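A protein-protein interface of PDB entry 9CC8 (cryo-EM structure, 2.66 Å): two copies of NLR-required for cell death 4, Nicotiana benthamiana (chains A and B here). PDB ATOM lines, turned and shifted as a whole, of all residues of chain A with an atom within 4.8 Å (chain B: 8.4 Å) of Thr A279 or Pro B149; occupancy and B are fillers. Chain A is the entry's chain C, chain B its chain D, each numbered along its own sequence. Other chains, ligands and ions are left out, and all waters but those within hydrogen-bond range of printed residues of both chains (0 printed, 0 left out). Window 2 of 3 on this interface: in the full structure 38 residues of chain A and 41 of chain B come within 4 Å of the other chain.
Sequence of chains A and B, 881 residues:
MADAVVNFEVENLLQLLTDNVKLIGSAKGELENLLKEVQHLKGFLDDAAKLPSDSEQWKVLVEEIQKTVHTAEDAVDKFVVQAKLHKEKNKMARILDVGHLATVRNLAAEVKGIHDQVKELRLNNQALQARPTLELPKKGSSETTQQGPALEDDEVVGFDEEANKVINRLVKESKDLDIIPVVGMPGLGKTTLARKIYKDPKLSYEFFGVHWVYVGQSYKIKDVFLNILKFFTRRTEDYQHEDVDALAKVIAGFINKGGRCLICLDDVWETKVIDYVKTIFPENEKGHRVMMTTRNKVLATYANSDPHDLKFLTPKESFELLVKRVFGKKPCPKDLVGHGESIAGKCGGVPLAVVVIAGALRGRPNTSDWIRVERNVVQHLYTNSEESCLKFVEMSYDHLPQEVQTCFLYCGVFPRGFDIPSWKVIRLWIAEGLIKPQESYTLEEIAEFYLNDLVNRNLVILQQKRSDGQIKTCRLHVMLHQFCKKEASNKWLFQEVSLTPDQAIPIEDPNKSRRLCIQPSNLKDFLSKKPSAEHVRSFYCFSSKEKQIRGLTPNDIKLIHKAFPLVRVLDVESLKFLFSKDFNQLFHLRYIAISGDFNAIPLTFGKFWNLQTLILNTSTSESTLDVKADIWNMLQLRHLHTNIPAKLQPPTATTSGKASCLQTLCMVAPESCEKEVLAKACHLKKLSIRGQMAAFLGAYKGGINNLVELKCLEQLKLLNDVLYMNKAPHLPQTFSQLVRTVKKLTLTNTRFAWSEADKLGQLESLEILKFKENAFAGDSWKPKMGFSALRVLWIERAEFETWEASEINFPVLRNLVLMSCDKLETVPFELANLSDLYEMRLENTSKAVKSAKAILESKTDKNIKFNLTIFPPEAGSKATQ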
ATOM      1  N   PHE A 225      40.337  19.114 -10.801  1.00  0.00           N
ATOM      2  CA  PHE A 225      40.509  20.373 -11.517  1.00  0.00           C
ATOM      3  C   PHE A 225      41.966  20.810 -11.526  1.00  0.00           C
ATOM      4  O   PHE A 225      42.463  21.300 -12.546  1.00  0.00           O
ATOM      5  CB  PHE A 225      39.631  21.453 -10.888  1.00  0.00           C
ATOM      6  CG  PHE A 225      38.180  21.391 -11.299  1.00  0.00           C
ATOM      7  CD1 PHE A 225      37.729  20.472 -12.234  1.00  0.00           C
ATOM      8  CD2 PHE A 225      37.264  22.262 -10.743  1.00  0.00           C
ATOM      9  CE1 PHE A 225      36.403  20.431 -12.600  1.00  0.00           C
ATOM     10  CE2 PHE A 225      35.937  22.221 -11.108  1.00  0.00           C
ATOM     11  CZ  PHE A 225      35.509  21.306 -12.037  1.00  0.00           C
ATOM     12  N   ALA A 248      37.442  26.206 -12.238  1.00  0.00           N
ATOM     13  CA  ALA A 248      36.716  25.886 -13.461  1.00  0.00           C
ATOM     14  C   ALA A 248      36.804  27.028 -14.458  1.00  0.00           C
ATOM     15  O   ALA A 248      37.024  26.803 -15.652  1.00  0.00           O
ATOM     16  CB  ALA A 248      35.257  25.576 -13.136  1.00  0.00           C
ATOM     17  N   ALA A 252      38.563  26.995 -18.080  1.00  0.00           N
ATOM     18  CA  ALA A 252      37.784  27.367 -19.251  1.00  0.00           C
ATOM     19  C   ALA A 252      38.501  28.431 -20.066  1.00  0.00           C
ATOM     20  O   ALA A 252      38.529  28.368 -21.298  1.00  0.00           O
ATOM     21  CB  ALA A 252      36.401  27.853 -18.823  1.00  0.00           C
ATOM     22  N   LYS A 272      27.910  13.589 -10.753  1.00  0.00           N
ATOM     23  CA  LYS A 272      28.455  14.850 -10.266  1.00  0.00           C
ATOM     24  C   LYS A 272      29.749  15.197 -10.984  1.00  0.00           C
ATOM     25  O   LYS A 272      30.025  16.371 -11.251  1.00  0.00           O
ATOM     26  CB  LYS A 272      28.686  14.757  -8.760  1.00  0.00           C
ATOM     27  CG  LYS A 272      28.678  16.082  -8.027  1.00  0.00           C
ATOM     28  CD  LYS A 272      28.675  15.856  -6.525  1.00  0.00           C
ATOM     29  CE  LYS A 272      28.808  17.155  -5.759  1.00  0.00           C
ATOM     30  NZ  LYS A 272      28.673  16.952  -4.293  1.00  0.00           N
ATOM     31  N   ASP A 275      28.842  16.634 -14.318  1.00  0.00           N
ATOM     32  CA  ASP A 275      28.338  17.998 -14.199  1.00  0.00           C
ATOM     33  C   ASP A 275      29.459  18.988 -13.905  1.00  0.00           C
ATOM     34  O   ASP A 275      29.480  20.090 -14.463  1.00  0.00           O
ATOM     35  CB  ASP A 275      27.268  18.062 -13.116  1.00  0.00           C
ATOM     36  CG  ASP A 275      26.058  17.240 -13.457  1.00  0.00           C
ATOM     37  OD1 ASP A 275      25.916  16.857 -14.635  1.00  0.00           O
ATOM     38  OD2 ASP A 275      25.248  16.972 -12.548  1.00  0.00           O
ATOM     39  N   TYR A 276      30.392  18.620 -13.027  1.00  0.00           N
ATOM     40  CA  TYR A 276      31.512  19.505 -12.730  1.00  0.00           C
ATOM     41  C   TYR A 276      32.362  19.748 -13.965  1.00  0.00           C
ATOM     42  O   TYR A 276      32.770  20.883 -14.235  1.00  0.00           O
ATOM     43  CB  TYR A 276      32.375  18.908 -11.627  1.00  0.00           C
ATOM     44  CG  TYR A 276      32.032  19.372 -10.240  1.00  0.00           C
ATOM     45  CD1 TYR A 276      32.375  20.643  -9.807  1.00  0.00           C
ATOM     46  CD2 TYR A 276      31.402  18.524  -9.345  1.00  0.00           C
ATOM     47  CE1 TYR A 276      32.077  21.063  -8.529  1.00  0.00           C
ATOM     48  CE2 TYR A 276      31.101  18.935  -8.071  1.00  0.00           C
ATOM     49  CZ  TYR A 276      31.439  20.205  -7.667  1.00  0.00           C
ATOM     50  OH  TYR A 276      31.137  20.615  -6.391  1.00  0.00           O
ATOM     51  N   VAL A 277      32.658  18.690 -14.721  1.00  0.00           N
ATOM     52  CA  VAL A 277      33.519  18.826 -15.885  1.00  0.00           C
ATOM     53  C   VAL A 277      32.848  19.620 -16.997  1.00  0.00           C
ATOM     54  O   VAL A 277      33.539  20.225 -17.820  1.00  0.00           O
ATOM     55  CB  VAL A 277      33.948  17.428 -16.365  1.00  0.00           C
ATOM     56  CG1 VAL A 277      34.528  17.482 -17.767  1.00  0.00           C
ATOM     57  CG2 VAL A 277      34.955  16.842 -15.395  1.00  0.00           C
ATOM     58  N   LYS A 278      31.518  19.643 -17.054  1.00  0.00           N
ATOM     59  CA  LYS A 278      30.852  20.471 -18.048  1.00  0.00           C
ATOM     60  C   LYS A 278      31.135  21.949 -17.841  1.00  0.00           C
ATOM     61  O   LYS A 278      30.983  22.735 -18.781  1.00  0.00           O
ATOM     62  CB  LYS A 278      29.344  20.237 -18.007  1.00  0.00           C
ATOM     63  CG  LYS A 278      28.887  18.950 -18.643  1.00  0.00           C
ATOM     64  CD  LYS A 278      27.452  18.671 -18.270  1.00  0.00           C
ATOM     65  CE  LYS A 278      26.885  17.498 -19.028  1.00  0.00           C
ATOM     66  NZ  LYS A 278      25.425  17.376 -18.798  1.00  0.00           N
ATOM     67  N   THR A 279      31.538  22.340 -16.635  1.00  0.00           N
ATOM     68  CA  THR A 279      31.737  23.740 -16.295  1.00  0.00           C
ATOM     69  C   THR A 279      33.125  24.254 -16.643  1.00  0.00           C
ATOM     70  O   THR A 279      33.359  25.461 -16.538  1.00  0.00           O
ATOM     71  CB  THR A 279      31.490  23.951 -14.801  1.00  0.00           C
ATOM     72  OG1 THR A 279      32.532  23.317 -14.051  1.00  0.00           O
ATOM     73  CG2 THR A 279      30.155  23.372 -14.393  1.00  0.00           C
ATOM     74  N   ILE A 280      34.053  23.380 -17.048  1.00  0.00           N
ATOM     75  CA  ILE A 280      35.403  23.813 -17.389  1.00  0.00           C
ATOM     76  C   ILE A 280      35.585  24.050 -18.877  1.00  0.00           C
ATOM     77  O   ILE A 280      36.704  24.343 -19.313  1.00  0.00           O
ATOM     78  CB  ILE A 280      36.456  22.792 -16.909  1.00  0.00           C
ATOM     79  CG1 ILE A 280      36.365  21.483 -17.698  1.00  0.00           C
ATOM     80  CG2 ILE A 280      36.270  22.511 -15.439  1.00  0.00           C
ATOM     81  CD1 ILE A 280      37.592  20.623 -17.589  1.00  0.00           C
ATOM     82  N   PHE A 281      34.529  23.922 -19.674  1.00  0.00           N
ATOM     83  CA  PHE A 281      34.638  24.059 -21.116  1.00  0.00           C
ATOM     84  C   PHE A 281      34.003  25.368 -21.555  1.00  0.00           C
ATOM     85  O   PHE A 281      32.806  25.576 -21.309  1.00  0.00           O
ATOM     86  CB  PHE A 281      33.971  22.880 -21.817  1.00  0.00           C
ATOM     87  CG  PHE A 281      34.758  21.614 -21.728  1.00  0.00           C
ATOM     88  CD1 PHE A 281      35.777  21.356 -22.622  1.00  0.00           C
ATOM     89  CD2 PHE A 281      34.496  20.689 -20.736  1.00  0.00           C
ATOM     90  CE1 PHE A 281      36.508  20.193 -22.541  1.00  0.00           C
ATOM     91  CE2 PHE A 281      35.225  19.528 -20.649  1.00  0.00           C
ATOM     92  CZ  PHE A 281      36.233  19.280 -21.553  1.00  0.00           C
ATOM     93  N   GLN B 146      30.719  21.796   0.781  1.00  0.00           N
ATOM     94  CA  GLN B 146      30.896  21.806  -0.666  1.00  0.00           C
ATOM     95  C   GLN B 146      29.552  22.019  -1.358  1.00  0.00           C
ATOM     96  O   GLN B 146      28.512  21.593  -0.855  1.00  0.00           O
ATOM     97  CB  GLN B 146      31.541  20.501  -1.136  1.00  0.00           C
ATOM     98  CG  GLN B 146      31.987  20.506  -2.590  1.00  0.00           C
ATOM     99  CD  GLN B 146      31.971  19.123  -3.205  1.00  0.00           C
ATOM    100  OE1 GLN B 146      31.018  18.745  -3.886  1.00  0.00           O
ATOM    101  NE2 GLN B 146      33.032  18.360  -2.971  1.00  0.00           N
ATOM    102  N   GLN B 147      29.583  22.687  -2.505  1.00  0.00           N
ATOM    103  CA  GLN B 147      28.398  22.995  -3.287  1.00  0.00           C
ATOM    104  C   GLN B 147      28.419  22.193  -4.587  1.00  0.00           C
ATOM    105  O   GLN B 147      29.288  21.341  -4.806  1.00  0.00           O
ATOM    106  CB  GLN B 147      28.323  24.501  -3.550  1.00  0.00           C
ATOM    107  CG  GLN B 147      28.399  25.360  -2.295  1.00  0.00           C
ATOM    108  CD  GLN B 147      27.041  25.863  -1.850  1.00  0.00           C
ATOM    109  OE1 GLN B 147      26.255  26.356  -2.660  1.00  0.00           O
ATOM    110  NE2 GLN B 147      26.756  25.740  -0.559  1.00  0.00           N
ATOM    111  N   GLY B 148      27.449  22.466  -5.459  1.00  0.00           N
ATOM    112  CA  GLY B 148      27.364  21.777  -6.722  1.00  0.00           C
ATOM    113  C   GLY B 148      28.339  22.331  -7.737  1.00  0.00           C
ATOM    114  O   GLY B 148      29.154  23.218  -7.454  1.00  0.00           O
ATOM    115  N   PRO B 149      28.278  21.782  -8.950  1.00  0.00           N
ATOM    116  CA  PRO B 149      29.139  22.273 -10.032  1.00  0.00           C
ATOM    117  C   PRO B 149      29.227  23.789 -10.117  1.00  0.00           C
ATOM    118  O   PRO B 149      30.325  24.341 -10.001  1.00  0.00           O
ATOM    119  CB  PRO B 149      28.492  21.677 -11.289  1.00  0.00           C
ATOM    120  CG  PRO B 149      27.597  20.566 -10.806  1.00  0.00           C
ATOM    121  CD  PRO B 149      27.631  20.514  -9.314  1.00  0.00           C
ATOM    122  N   ALA B 150      28.080  24.456 -10.277  1.00  0.00           N
ATOM    123  CA  ALA B 150      27.973  25.892 -10.539  1.00  0.00           C
ATOM    124  C   ALA B 150      26.987  26.119 -11.672  1.00  0.00           C
ATOM    125  O   ALA B 150      27.142  25.555 -12.759  1.00  0.00           O
ATOM    126  CB  ALA B 150      29.313  26.530 -10.903  1.00  0.00           C
ATOM    127  N   LEU B 151      25.972  26.938 -11.431  1.00  0.00           N
ATOM    128  CA  LEU B 151      24.879  27.107 -12.373  1.00  0.00           C
ATOM    129  C   LEU B 151      25.165  28.259 -13.321  1.00  0.00           C
ATOM    130  O   LEU B 151      25.502  29.361 -12.886  1.00  0.00           O
ATOM    131  CB  LEU B 151      23.572  27.355 -11.626  1.00  0.00           C
ATOM    132  CG  LEU B 151      22.781  26.109 -11.245  1.00  0.00           C
ATOM    133  CD1 LEU B 151      23.653  25.135 -10.480  1.00  0.00           C
ATOM    134  CD2 LEU B 151      21.583  26.513 -10.422  1.00  0.00           C
ATOM    135  N   GLU B 152      25.040  27.994 -14.614  1.00  0.00           N
ATOM    136  CA  GLU B 152      24.995  29.061 -15.596  1.00  0.00           C
ATOM    137  C   GLU B 152      23.618  29.701 -15.551  1.00  0.00           C
ATOM    138  O   GLU B 152      22.617  29.027 -15.302  1.00  0.00           O
ATOM    139  CB  GLU B 152      25.295  28.523 -16.994  1.00  0.00           C
ATOM    140  CG  GLU B 152      26.499  27.589 -17.050  1.00  0.00           C
ATOM    141  CD  GLU B 152      27.778  28.242 -16.547  1.00  0.00           C
ATOM    142  OE1 GLU B 152      27.798  29.478 -16.382  1.00  0.00           O
ATOM    143  OE2 GLU B 152      28.765  27.513 -16.311  1.00  0.00           O
ATOM    144  N   GLU B 155      20.664  27.884 -16.402  1.00  0.00           N
ATOM    145  CA  GLU B 155      20.294  26.710 -15.626  1.00  0.00           C
ATOM    146  C   GLU B 155      19.434  27.044 -14.418  1.00  0.00           C
ATOM    147  O   GLU B 155      18.927  26.124 -13.771  1.00  0.00           O
ATOM    148  CB  GLU B 155      21.541  25.965 -15.151  1.00  0.00           C
ATOM    149  CG  GLU B 155      22.336  25.310 -16.254  1.00  0.00           C
ATOM    150  CD  GLU B 155      23.613  24.682 -15.745  1.00  0.00           C
ATOM    151  OE1 GLU B 155      23.728  24.467 -14.525  1.00  0.00           O
ATOM    152  OE2 GLU B 155      24.512  24.415 -16.565  1.00  0.00           O
ATOM    153  N   ARG B 325      17.821  19.289 -15.162  1.00  0.00           N
ATOM    154  CA  ARG B 325      18.728  18.470 -14.370  1.00  0.00           C
ATOM    155  C   ARG B 325      18.897  17.075 -14.945  1.00  0.00           C
ATOM    156  O   ARG B 325      19.979  16.493 -14.827  1.00  0.00           O
ATOM    157  CB  ARG B 325      18.228  18.372 -12.931  1.00  0.00           C
ATOM    158  CG  ARG B 325      18.244  19.679 -12.183  1.00  0.00           C
ATOM    159  CD  ARG B 325      19.619  19.999 -11.655  1.00  0.00           C
ATOM    160  NE  ARG B 325      19.737  21.413 -11.324  1.00  0.00           N
ATOM    161  CZ  ARG B 325      20.602  21.918 -10.457  1.00  0.00           C
ATOM    162  NH1 ARG B 325      21.466  21.154  -9.814  1.00  0.00           N
ATOM    163  NH2 ARG B 325      20.603  23.224 -10.233  1.00  0.00           N
ATOM    164  N   VAL B 355      16.058  18.494  -7.598  1.00  0.00           N
ATOM    165  CA  VAL B 355      17.423  18.074  -7.904  1.00  0.00           C
ATOM    166  C   VAL B 355      17.651  16.633  -7.461  1.00  0.00           C
ATOM    167  O   VAL B 355      18.251  15.828  -8.185  1.00  0.00           O
ATOM    168  CB  VAL B 355      18.429  19.038  -7.247  1.00  0.00           C
ATOM    169  CG1 VAL B 355      19.835  18.502  -7.359  1.00  0.00           C
ATOM    170  CG2 VAL B 355      18.331  20.420  -7.875  1.00  0.00           C
ATOM    171  N   ARG B 362      18.241  10.296 -13.529  1.00  0.00           N
ATOM    172  CA  ARG B 362      19.307  10.612 -14.471  1.00  0.00           C
ATOM    173  C   ARG B 362      19.774   9.359 -15.193  1.00  0.00           C
ATOM    174  O   ARG B 362      20.148   8.368 -14.561  1.00  0.00           O
ATOM    175  CB  ARG B 362      20.480  11.264 -13.747  1.00  0.00           C
ATOM    176  CG  ARG B 362      20.513  12.759 -13.893  1.00  0.00           C
ATOM    177  CD  ARG B 362      21.453  13.391 -12.904  1.00  0.00           C
ATOM    178  NE  ARG B 362      21.387  14.844 -12.969  1.00  0.00           N
ATOM    179  CZ  ARG B 362      22.412  15.654 -12.749  1.00  0.00           C
ATOM    180  NH1 ARG B 362      23.597  15.192 -12.387  1.00  0.00           N
ATOM    181  NH2 ARG B 362      22.242  16.966 -12.890  1.00  0.00           N
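Hydrophobic or aromatic side chains of chain B within 4 Å of the printed part of chain A: Pro B149.
Printed residues of chain A that touch a printed residue of chain B: Lys A272, Asp A275, Tyr A276 and Thr A279.
Among the printed residues, 8 pairs touch across the chains.
Among the printed residues, Asp or Glu carboxylates within 4 Å of a Lys or Arg side-chain nitrogen of the other chain: Asp A275 with Arg B362.
CB of Asp A275 touches CG of Pro B149, 3.4 Å away.
Pro B149 touches Tyr A276.
CB of Pro B149 touches CG2 of Thr A279 (3.9 Å).
NZ of Lys A272 sits at hydrogen-bond distance from OE1 of Gln B146 (3.0 Å).
The guanidinium group of Arg B362 lies within salt-bridge range of the side-chain carboxylate of Asp A275, at 2.4 Å.
OE1 of Gln B146 lies within hydrogen-bond range of OH of Tyr A276 (3.1 Å).
The side-chain hydroxyl of Tyr A276 sits at hydrogen-bond distance from the backbone carbonyl oxygen of Gln B147 (2.5 Å).
OH of Tyr A276 lies within hydrogen-bond range of O of Gly B148 (3.4 Å).
Printed residues of chain B within 4 Å of Lys A272: Gln B146 (3.0 Å).
Of the printed residues of chain B, Tyr A276 touches Gln B146, Gln B147, Gly B148 and Pro B149.
Thr A279 touches just one residue of chain B: Pro B149 (3.9 Å).
Of the printed residues of chain A, Gln B146 touches Lys A272 (3.0 Å) and Tyr A276 (3.1 Å).
Of the printed residues of chain A, Gly B148 touches Tyr A276 (3.4 Å).
Of the printed residues of chain A, Pro B149 touches Asp A275 (3.4 Å), Tyr A276 (3.5 Å) and Thr A279 (3.9 Å).
Arg B325 touches none of the printed residues of chain A.
The nearest residue of chain B that does not touch Thr A279 is Ala B150 (4.1 Å).
The nearest printed residue of chain A that does not touch Gln B147 is Lys A272 (4.3 Å).
No position is printed for both chains.
Of the 8 pairs that touch across the chains among the printed residues, none has its exchanged pair printed and touching as well.
O of Tyr A276 sits at hydrogen-bond distance from OG1 of Thr A279 (2.5 Å).
The guanidinium group (NE) of Arg B362 lies within hydrogen-bond range of the backbone carbonyl oxygen (O) of Arg B325, 2.9 Å away.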
